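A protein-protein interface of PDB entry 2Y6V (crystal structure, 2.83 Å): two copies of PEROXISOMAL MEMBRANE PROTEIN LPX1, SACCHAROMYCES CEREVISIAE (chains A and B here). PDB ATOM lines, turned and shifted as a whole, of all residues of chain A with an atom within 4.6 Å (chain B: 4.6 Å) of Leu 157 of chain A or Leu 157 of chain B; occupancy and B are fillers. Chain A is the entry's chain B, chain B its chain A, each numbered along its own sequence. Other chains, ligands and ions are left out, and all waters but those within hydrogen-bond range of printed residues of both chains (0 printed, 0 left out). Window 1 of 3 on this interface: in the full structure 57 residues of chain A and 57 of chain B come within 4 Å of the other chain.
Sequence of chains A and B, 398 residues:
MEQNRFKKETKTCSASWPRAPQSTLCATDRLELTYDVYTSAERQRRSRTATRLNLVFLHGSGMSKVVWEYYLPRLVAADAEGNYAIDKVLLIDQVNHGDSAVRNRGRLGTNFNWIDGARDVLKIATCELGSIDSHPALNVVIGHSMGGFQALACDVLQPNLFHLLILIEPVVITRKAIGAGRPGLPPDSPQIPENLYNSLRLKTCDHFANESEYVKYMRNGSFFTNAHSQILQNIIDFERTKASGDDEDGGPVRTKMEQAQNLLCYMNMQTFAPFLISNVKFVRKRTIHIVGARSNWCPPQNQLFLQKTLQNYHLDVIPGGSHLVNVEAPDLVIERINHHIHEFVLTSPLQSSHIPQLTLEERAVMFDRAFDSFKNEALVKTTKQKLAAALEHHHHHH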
ATOM      1  N   ILE A 115      22.704 -16.119   9.987  1.00  0.00           N
ATOM      2  CA  ILE A 115      23.409 -15.215   9.092  1.00  0.00           C
ATOM      3  C   ILE A 115      24.710 -15.924   8.672  1.00  0.00           C
ATOM      4  O   ILE A 115      25.108 -15.858   7.510  1.00  0.00           O
ATOM      5  CB  ILE A 115      23.667 -13.813   9.729  1.00  0.00           C
ATOM      6  CG1 ILE A 115      22.371 -13.172  10.213  1.00  0.00           C
ATOM      7  CG2 ILE A 115      24.264 -12.896   8.742  1.00  0.00           C
ATOM      8  CD1 ILE A 115      22.559 -11.908  11.039  1.00  0.00           C
ATOM      9  N   ARG A 119      26.044 -16.584   4.923  1.00  0.00           N
ATOM     10  CA  ARG A 119      27.430 -16.411   4.408  1.00  0.00           C
ATOM     11  C   ARG A 119      27.960 -17.661   3.647  1.00  0.00           C
ATOM     12  O   ARG A 119      28.802 -17.541   2.761  1.00  0.00           O
ATOM     13  CB  ARG A 119      28.423 -15.944   5.513  1.00  0.00           C
ATOM     14  CG  ARG A 119      28.292 -14.465   5.858  1.00  0.00           C
ATOM     15  CD  ARG A 119      29.416 -13.852   6.714  1.00  0.00           C
ATOM     16  NE  ARG A 119      29.121 -14.152   8.091  1.00  0.00           N
ATOM     17  CZ  ARG A 119      28.462 -13.394   8.940  1.00  0.00           C
ATOM     18  NH1 ARG A 119      28.096 -12.208   8.629  1.00  0.00           N
ATOM     19  NH2 ARG A 119      28.194 -13.844  10.131  1.00  0.00           N
ATOM     20  N   LEU A 122      26.173 -17.543   0.161  1.00  0.00           N
ATOM     21  CA  LEU A 122      26.888 -16.602  -0.710  1.00  0.00           C
ATOM     22  C   LEU A 122      28.180 -17.210  -1.224  1.00  0.00           C
ATOM     23  O   LEU A 122      28.462 -17.118  -2.399  1.00  0.00           O
ATOM     24  CB  LEU A 122      27.193 -15.268  -0.010  1.00  0.00           C
ATOM     25  CG  LEU A 122      25.958 -14.437   0.317  1.00  0.00           C
ATOM     26  CD1 LEU A 122      26.304 -13.153   1.059  1.00  0.00           C
ATOM     27  CD2 LEU A 122      25.175 -14.147  -0.977  1.00  0.00           C
ATOM     28  N   ALA A 153      18.879 -12.362   4.057  1.00  0.00           N
ATOM     29  CA  ALA A 153      20.221 -12.010   4.591  1.00  0.00           C
ATOM     30  C   ALA A 153      21.260 -11.965   3.466  1.00  0.00           C
ATOM     31  O   ALA A 153      22.164 -11.121   3.502  1.00  0.00           O
ATOM     32  CB  ALA A 153      20.675 -12.962   5.754  1.00  0.00           C
ATOM     33  N   CYS A 154      21.116 -12.852   2.479  1.00  0.00           N
ATOM     34  CA  CYS A 154      22.053 -12.907   1.348  1.00  0.00           C
ATOM     35  C   CYS A 154      22.064 -11.568   0.602  1.00  0.00           C
ATOM     36  O   CYS A 154      23.116 -11.013   0.284  1.00  0.00           O
ATOM     37  CB  CYS A 154      21.703 -14.035   0.368  1.00  0.00           C
ATOM     38  SG  CYS A 154      22.115 -15.733   0.916  1.00  0.00           S
ATOM     39  N   ASP A 155      20.881 -11.024   0.355  1.00  0.00           N
ATOM     40  CA  ASP A 155      20.797  -9.729  -0.317  1.00  0.00           C
ATOM     41  C   ASP A 155      21.418  -8.586   0.514  1.00  0.00           C
ATOM     42  O   ASP A 155      22.133  -7.740  -0.010  1.00  0.00           O
ATOM     43  CB  ASP A 155      19.366  -9.389  -0.713  1.00  0.00           C
ATOM     44  CG  ASP A 155      19.319  -8.338  -1.804  1.00  0.00           C
ATOM     45  OD1 ASP A 155      19.646  -8.705  -2.937  1.00  0.00           O
ATOM     46  OD2 ASP A 155      19.001  -7.162  -1.553  1.00  0.00           O
ATOM     47  N   VAL A 156      21.176  -8.610   1.819  1.00  0.00           N
ATOM     48  CA  VAL A 156      21.687  -7.598   2.737  1.00  0.00           C
ATOM     49  C   VAL A 156      23.196  -7.584   2.698  1.00  0.00           C
ATOM     50  O   VAL A 156      23.791  -6.532   2.471  1.00  0.00           O
ATOM     51  CB  VAL A 156      21.187  -7.808   4.170  1.00  0.00           C
ATOM     52  CG1 VAL A 156      21.941  -6.898   5.114  1.00  0.00           C
ATOM     53  CG2 VAL A 156      19.674  -7.540   4.240  1.00  0.00           C
ATOM     54  N   LEU A 157      23.803  -8.760   2.825  1.00  0.00           N
ATOM     55  CA  LEU A 157      25.266  -8.879   2.831  1.00  0.00           C
ATOM     56  C   LEU A 157      25.938  -8.742   1.432  1.00  0.00           C
ATOM     57  O   LEU A 157      27.139  -8.464   1.328  1.00  0.00           O
ATOM     58  CB  LEU A 157      25.660 -10.210   3.481  1.00  0.00           C
ATOM     59  CG  LEU A 157      25.274 -10.485   4.928  1.00  0.00           C
ATOM     60  CD1 LEU A 157      25.692 -11.918   5.292  1.00  0.00           C
ATOM     61  CD2 LEU A 157      25.921  -9.450   5.796  1.00  0.00           C
ATOM     62  N   GLN A 158      25.170  -8.950   0.370  1.00  0.00           N
ATOM     63  CA  GLN A 158      25.676  -8.955  -1.007  1.00  0.00           C
ATOM     64  C   GLN A 158      24.524  -8.637  -1.981  1.00  0.00           C
ATOM     65  O   GLN A 158      23.961  -9.539  -2.596  1.00  0.00           O
ATOM     66  CB  GLN A 158      26.263 -10.334  -1.322  1.00  0.00           C
ATOM     67  CG  GLN A 158      26.760 -10.551  -2.760  1.00  0.00           C
ATOM     68  CD  GLN A 158      27.517  -9.358  -3.337  1.00  0.00           C
ATOM     69  OE1 GLN A 158      26.916  -8.376  -3.730  1.00  0.00           O
ATOM     70  NE2 GLN A 158      28.826  -9.451  -3.404  1.00  0.00           N
ATOM     71  N   PRO A 159      24.173  -7.345  -2.125  1.00  0.00           N
ATOM     72  CA  PRO A 159      22.990  -6.929  -2.843  1.00  0.00           C
ATOM     73  C   PRO A 159      23.097  -6.996  -4.393  1.00  0.00           C
ATOM     74  O   PRO A 159      22.174  -6.596  -5.072  1.00  0.00           O
ATOM     75  CB  PRO A 159      22.807  -5.496  -2.340  1.00  0.00           C
ATOM     76  CG  PRO A 159      24.168  -5.000  -2.157  1.00  0.00           C
ATOM     77  CD  PRO A 159      24.939  -6.177  -1.647  1.00  0.00           C
ATOM     78  N   PHE A 275      19.431  -8.046  13.674  1.00  0.00           N
ATOM     79  CA  PHE A 275      20.274  -7.501  12.601  1.00  0.00           C
ATOM     80  C   PHE A 275      19.549  -7.537  11.268  1.00  0.00           C
ATOM     81  O   PHE A 275      19.567  -6.547  10.545  1.00  0.00           O
ATOM     82  CB  PHE A 275      21.600  -8.227  12.479  1.00  0.00           C
ATOM     83  CG  PHE A 275      22.430  -7.771  11.329  1.00  0.00           C
ATOM     84  CD1 PHE A 275      23.291  -6.714  11.455  1.00  0.00           C
ATOM     85  CD2 PHE A 275      22.370  -8.423  10.122  1.00  0.00           C
ATOM     86  CE1 PHE A 275      24.078  -6.328  10.380  1.00  0.00           C
ATOM     87  CE2 PHE A 275      23.150  -8.033   9.058  1.00  0.00           C
ATOM     88  CZ  PHE A 275      24.003  -6.987   9.192  1.00  0.00           C
ATOM     89  N   ILE B 115      31.648  -0.115   0.191  1.00  0.00           N
ATOM     90  CA  ILE B 115      31.270  -1.405   0.830  1.00  0.00           C
ATOM     91  C   ILE B 115      31.809  -2.562  -0.018  1.00  0.00           C
ATOM     92  O   ILE B 115      32.312  -3.539   0.546  1.00  0.00           O
ATOM     93  CB  ILE B 115      29.729  -1.575   1.108  1.00  0.00           C
ATOM     94  CG1 ILE B 115      29.217  -0.408   1.942  1.00  0.00           C
ATOM     95  CG2 ILE B 115      29.455  -2.834   1.857  1.00  0.00           C
ATOM     96  CD1 ILE B 115      27.701  -0.340   2.075  1.00  0.00           C
ATOM     97  N   ARG B 119      34.282  -5.576   1.210  1.00  0.00           N
ATOM     98  CA  ARG B 119      34.183  -7.003   0.850  1.00  0.00           C
ATOM     99  C   ARG B 119      35.552  -7.538   0.362  1.00  0.00           C
ATOM    100  O   ARG B 119      35.849  -8.737   0.554  1.00  0.00           O
ATOM    101  CB  ARG B 119      33.026  -7.301  -0.139  1.00  0.00           C
ATOM    102  CG  ARG B 119      31.674  -7.287   0.529  1.00  0.00           C
ATOM    103  CD  ARG B 119      30.527  -7.859  -0.355  1.00  0.00           C
ATOM    104  NE  ARG B 119      30.032  -6.821  -1.224  1.00  0.00           N
ATOM    105  CZ  ARG B 119      29.065  -5.971  -0.928  1.00  0.00           C
ATOM    106  NH1 ARG B 119      28.362  -6.052   0.191  1.00  0.00           N
ATOM    107  NH2 ARG B 119      28.777  -5.024  -1.785  1.00  0.00           N
ATOM    108  N   LEU B 122      37.751  -8.173   3.449  1.00  0.00           N
ATOM    109  CA  LEU B 122      37.362  -9.397   4.154  1.00  0.00           C
ATOM    110  C   LEU B 122      37.903 -10.589   3.403  1.00  0.00           C
ATOM    111  O   LEU B 122      38.416 -11.510   4.002  1.00  0.00           O
ATOM    112  CB  LEU B 122      35.838  -9.506   4.336  1.00  0.00           C
ATOM    113  CG  LEU B 122      35.191  -8.463   5.258  1.00  0.00           C
ATOM    114  CD1 LEU B 122      33.693  -8.628   5.245  1.00  0.00           C
ATOM    115  CD2 LEU B 122      35.726  -8.517   6.682  1.00  0.00           C
ATOM    116  N   ALA B 153      32.612  -1.145   8.096  1.00  0.00           N
ATOM    117  CA  ALA B 153      31.796  -1.977   7.185  1.00  0.00           C
ATOM    118  C   ALA B 153      32.215  -3.457   7.246  1.00  0.00           C
ATOM    119  O   ALA B 153      31.343  -4.349   7.112  1.00  0.00           O
ATOM    120  CB  ALA B 153      31.833  -1.456   5.762  1.00  0.00           C
ATOM    121  N   CYS B 154      33.518  -3.708   7.464  1.00  0.00           N
ATOM    122  CA  CYS B 154      34.030  -5.056   7.616  1.00  0.00           C
ATOM    123  C   CYS B 154      33.403  -5.772   8.800  1.00  0.00           C
ATOM    124  O   CYS B 154      33.016  -6.926   8.696  1.00  0.00           O
ATOM    125  CB  CYS B 154      35.550  -5.059   7.801  1.00  0.00           C
ATOM    126  SG  CYS B 154      36.524  -4.738   6.269  1.00  0.00           S
ATOM    127  N   ASP B 155      33.324  -5.092   9.934  1.00  0.00           N
ATOM    128  CA  ASP B 155      32.710  -5.672  11.112  1.00  0.00           C
ATOM    129  C   ASP B 155      31.224  -5.936  10.859  1.00  0.00           C
ATOM    130  O   ASP B 155      30.729  -6.984  11.253  1.00  0.00           O
ATOM    131  CB  ASP B 155      32.923  -4.795  12.355  1.00  0.00           C
ATOM    132  CG  ASP B 155      32.720  -5.557  13.628  1.00  0.00           C
ATOM    133  OD1 ASP B 155      33.542  -6.430  13.914  1.00  0.00           O
ATOM    134  OD2 ASP B 155      31.726  -5.301  14.338  1.00  0.00           O
ATOM    135  N   VAL B 156      30.533  -5.009  10.186  1.00  0.00           N
ATOM    136  CA  VAL B 156      29.077  -5.125   9.951  1.00  0.00           C
ATOM    137  C   VAL B 156      28.788  -6.382   9.152  1.00  0.00           C
ATOM    138  O   VAL B 156      27.927  -7.165   9.512  1.00  0.00           O
ATOM    139  CB  VAL B 156      28.492  -3.870   9.267  1.00  0.00           C
ATOM    140  CG1 VAL B 156      27.055  -4.139   8.831  1.00  0.00           C
ATOM    141  CG2 VAL B 156      28.552  -2.684  10.203  1.00  0.00           C
ATOM    142  N   LEU B 157      29.558  -6.582   8.093  1.00  0.00           N
ATOM    143  CA  LEU B 157      29.356  -7.696   7.170  1.00  0.00           C
ATOM    144  C   LEU B 157      29.900  -9.030   7.686  1.00  0.00           C
ATOM    145  O   LEU B 157      29.551 -10.083   7.127  1.00  0.00           O
ATOM    146  CB  LEU B 157      30.019  -7.367   5.817  1.00  0.00           C
ATOM    147  CG  LEU B 157      29.457  -6.197   5.013  1.00  0.00           C
ATOM    148  CD1 LEU B 157      30.287  -5.934   3.817  1.00  0.00           C
ATOM    149  CD2 LEU B 157      28.055  -6.486   4.609  1.00  0.00           C
ATOM    150  N   GLN B 158      30.782  -8.962   8.699  1.00  0.00           N
ATOM    151  CA  GLN B 158      31.524 -10.102   9.266  1.00  0.00           C
ATOM    152  C   GLN B 158      32.019  -9.717  10.667  1.00  0.00           C
ATOM    153  O   GLN B 158      33.166  -9.336  10.845  1.00  0.00           O
ATOM    154  CB  GLN B 158      32.714 -10.470   8.361  1.00  0.00           C
ATOM    155  CG  GLN B 158      33.626 -11.609   8.843  1.00  0.00           C
ATOM    156  CD  GLN B 158      32.891 -12.800   9.361  1.00  0.00           C
ATOM    157  OE1 GLN B 158      32.524 -12.859  10.546  1.00  0.00           O
ATOM    158  NE2 GLN B 158      32.689 -13.779   8.496  1.00  0.00           N
ATOM    159  N   PRO B 159      31.134  -9.813  11.668  1.00  0.00           N
ATOM    160  CA  PRO B 159      31.417  -9.358  13.015  1.00  0.00           C
ATOM    161  C   PRO B 159      32.284 -10.308  13.890  1.00  0.00           C
ATOM    162  O   PRO B 159      32.415 -10.068  15.072  1.00  0.00           O
ATOM    163  CB  PRO B 159      29.997  -9.225  13.583  1.00  0.00           C
ATOM    164  CG  PRO B 159      29.258 -10.315  12.975  1.00  0.00           C
ATOM    165  CD  PRO B 159      29.773 -10.390  11.589  1.00  0.00           C
ATOM    166  N   PHE B 275      23.622   2.820   4.271  1.00  0.00           N
ATOM    167  CA  PHE B 275      23.644   1.438   4.744  1.00  0.00           C
ATOM    168  C   PHE B 275      24.554   1.285   5.928  1.00  0.00           C
ATOM    169  O   PHE B 275      24.188   0.633   6.879  1.00  0.00           O
ATOM    170  CB  PHE B 275      24.059   0.471   3.658  1.00  0.00           C
ATOM    171  CG  PHE B 275      24.211  -0.955   4.138  1.00  0.00           C
ATOM    172  CD1 PHE B 275      23.143  -1.820   4.129  1.00  0.00           C
ATOM    173  CD2 PHE B 275      25.438  -1.433   4.600  1.00  0.00           C
ATOM    174  CE1 PHE B 275      23.308  -3.138   4.576  1.00  0.00           C
ATOM    175  CE2 PHE B 275      25.581  -2.714   5.036  1.00  0.00           C
ATOM    176  CZ  PHE B 275      24.521  -3.568   5.035  1.00  0.00           C
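The guanidinium group of Arg 119 of chain B lies within hydrogen-bond range of the backbone carbonyl oxygen of Leu 157 of chain A (2.9 Å).
NH1 of Arg 119 of chain A lies within hydrogen-bond range of O of Leu 157 of chain B, 3.0 Å away.
Arg 119 of chain A touches Gln 158 of chain B.
Arg 119 of chain A touches Pro 159 of chain B.
O of Val 156 of chain A touches CZ of Phe 275 of chain B, at 3.99 Å.
Leu 157 of chain B touches Leu 157 of chain A.
NE of Arg 119 of chain B touches NE2 of Gln 158 of chain A, at 3.6 Å.
CD of Pro 159 of chain A touches NH1 of Arg 119 of chain B, 3.9 Å away.
Val 156 of chain B touches Phe 275 of chain A (O to CZ, 3.9 Å).
Of the printed residues of chain B, Arg 119 of chain A touches Leu 157, Gln 158 and Pro 159.
Cys 154 of chain A touches none of the printed residues of chain B.
Leu 157 of chain A touches just these residues of chain B: Arg 119 and Leu 157.
Printed residues of chain A within 4 Å of Arg 119 of chain B: Leu 157 (2.9 Å), Gln 158 (3.6 Å) and Pro 159 (3.9 Å).
Printed residues of chain A within 4 Å of Leu 157 of chain B: Arg 119 (3.0 Å) and Leu 157 (3.8 Å).
The nearest printed residue of chain A that does not touch Leu 157 of chain B is Val 156 of chain A (4.8 Å).
Along chain A the printed residues that touch a printed residue of chain B span positions 119 to 275.
Hydrophobic or aromatic side chains of chain B that line the printed part of chain A: Leu 157, Pro 159 and Phe 275.
Among the printed residues, 9 pairs touch across the chains.
Among the printed residues, no Asp or Glu carboxylate lies within 4 Å of a Lys or Arg side-chain nitrogen of the other chain.
Arg 119 of chain A touches Leu 157 of chain B, and with the chains exchanged Leu 157 of chain A touches Arg 119 of chain B.
Arg 119 of chain A touches Pro 159 of chain B, and with the chains exchanged Pro 159 of chain A touches Arg 119 of chain B.
Val 156 of chain A touches Phe 275 of chain B, and with the chains exchanged Phe 275 of chain A touches Val 156 of chain B.
Leu 157 of chain A touches its own counterpart, Leu 157 of chain B.
Of the 9 pairs that touch across the chains among the printed residues, 9 have their exchanged pair printed and touching as well.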
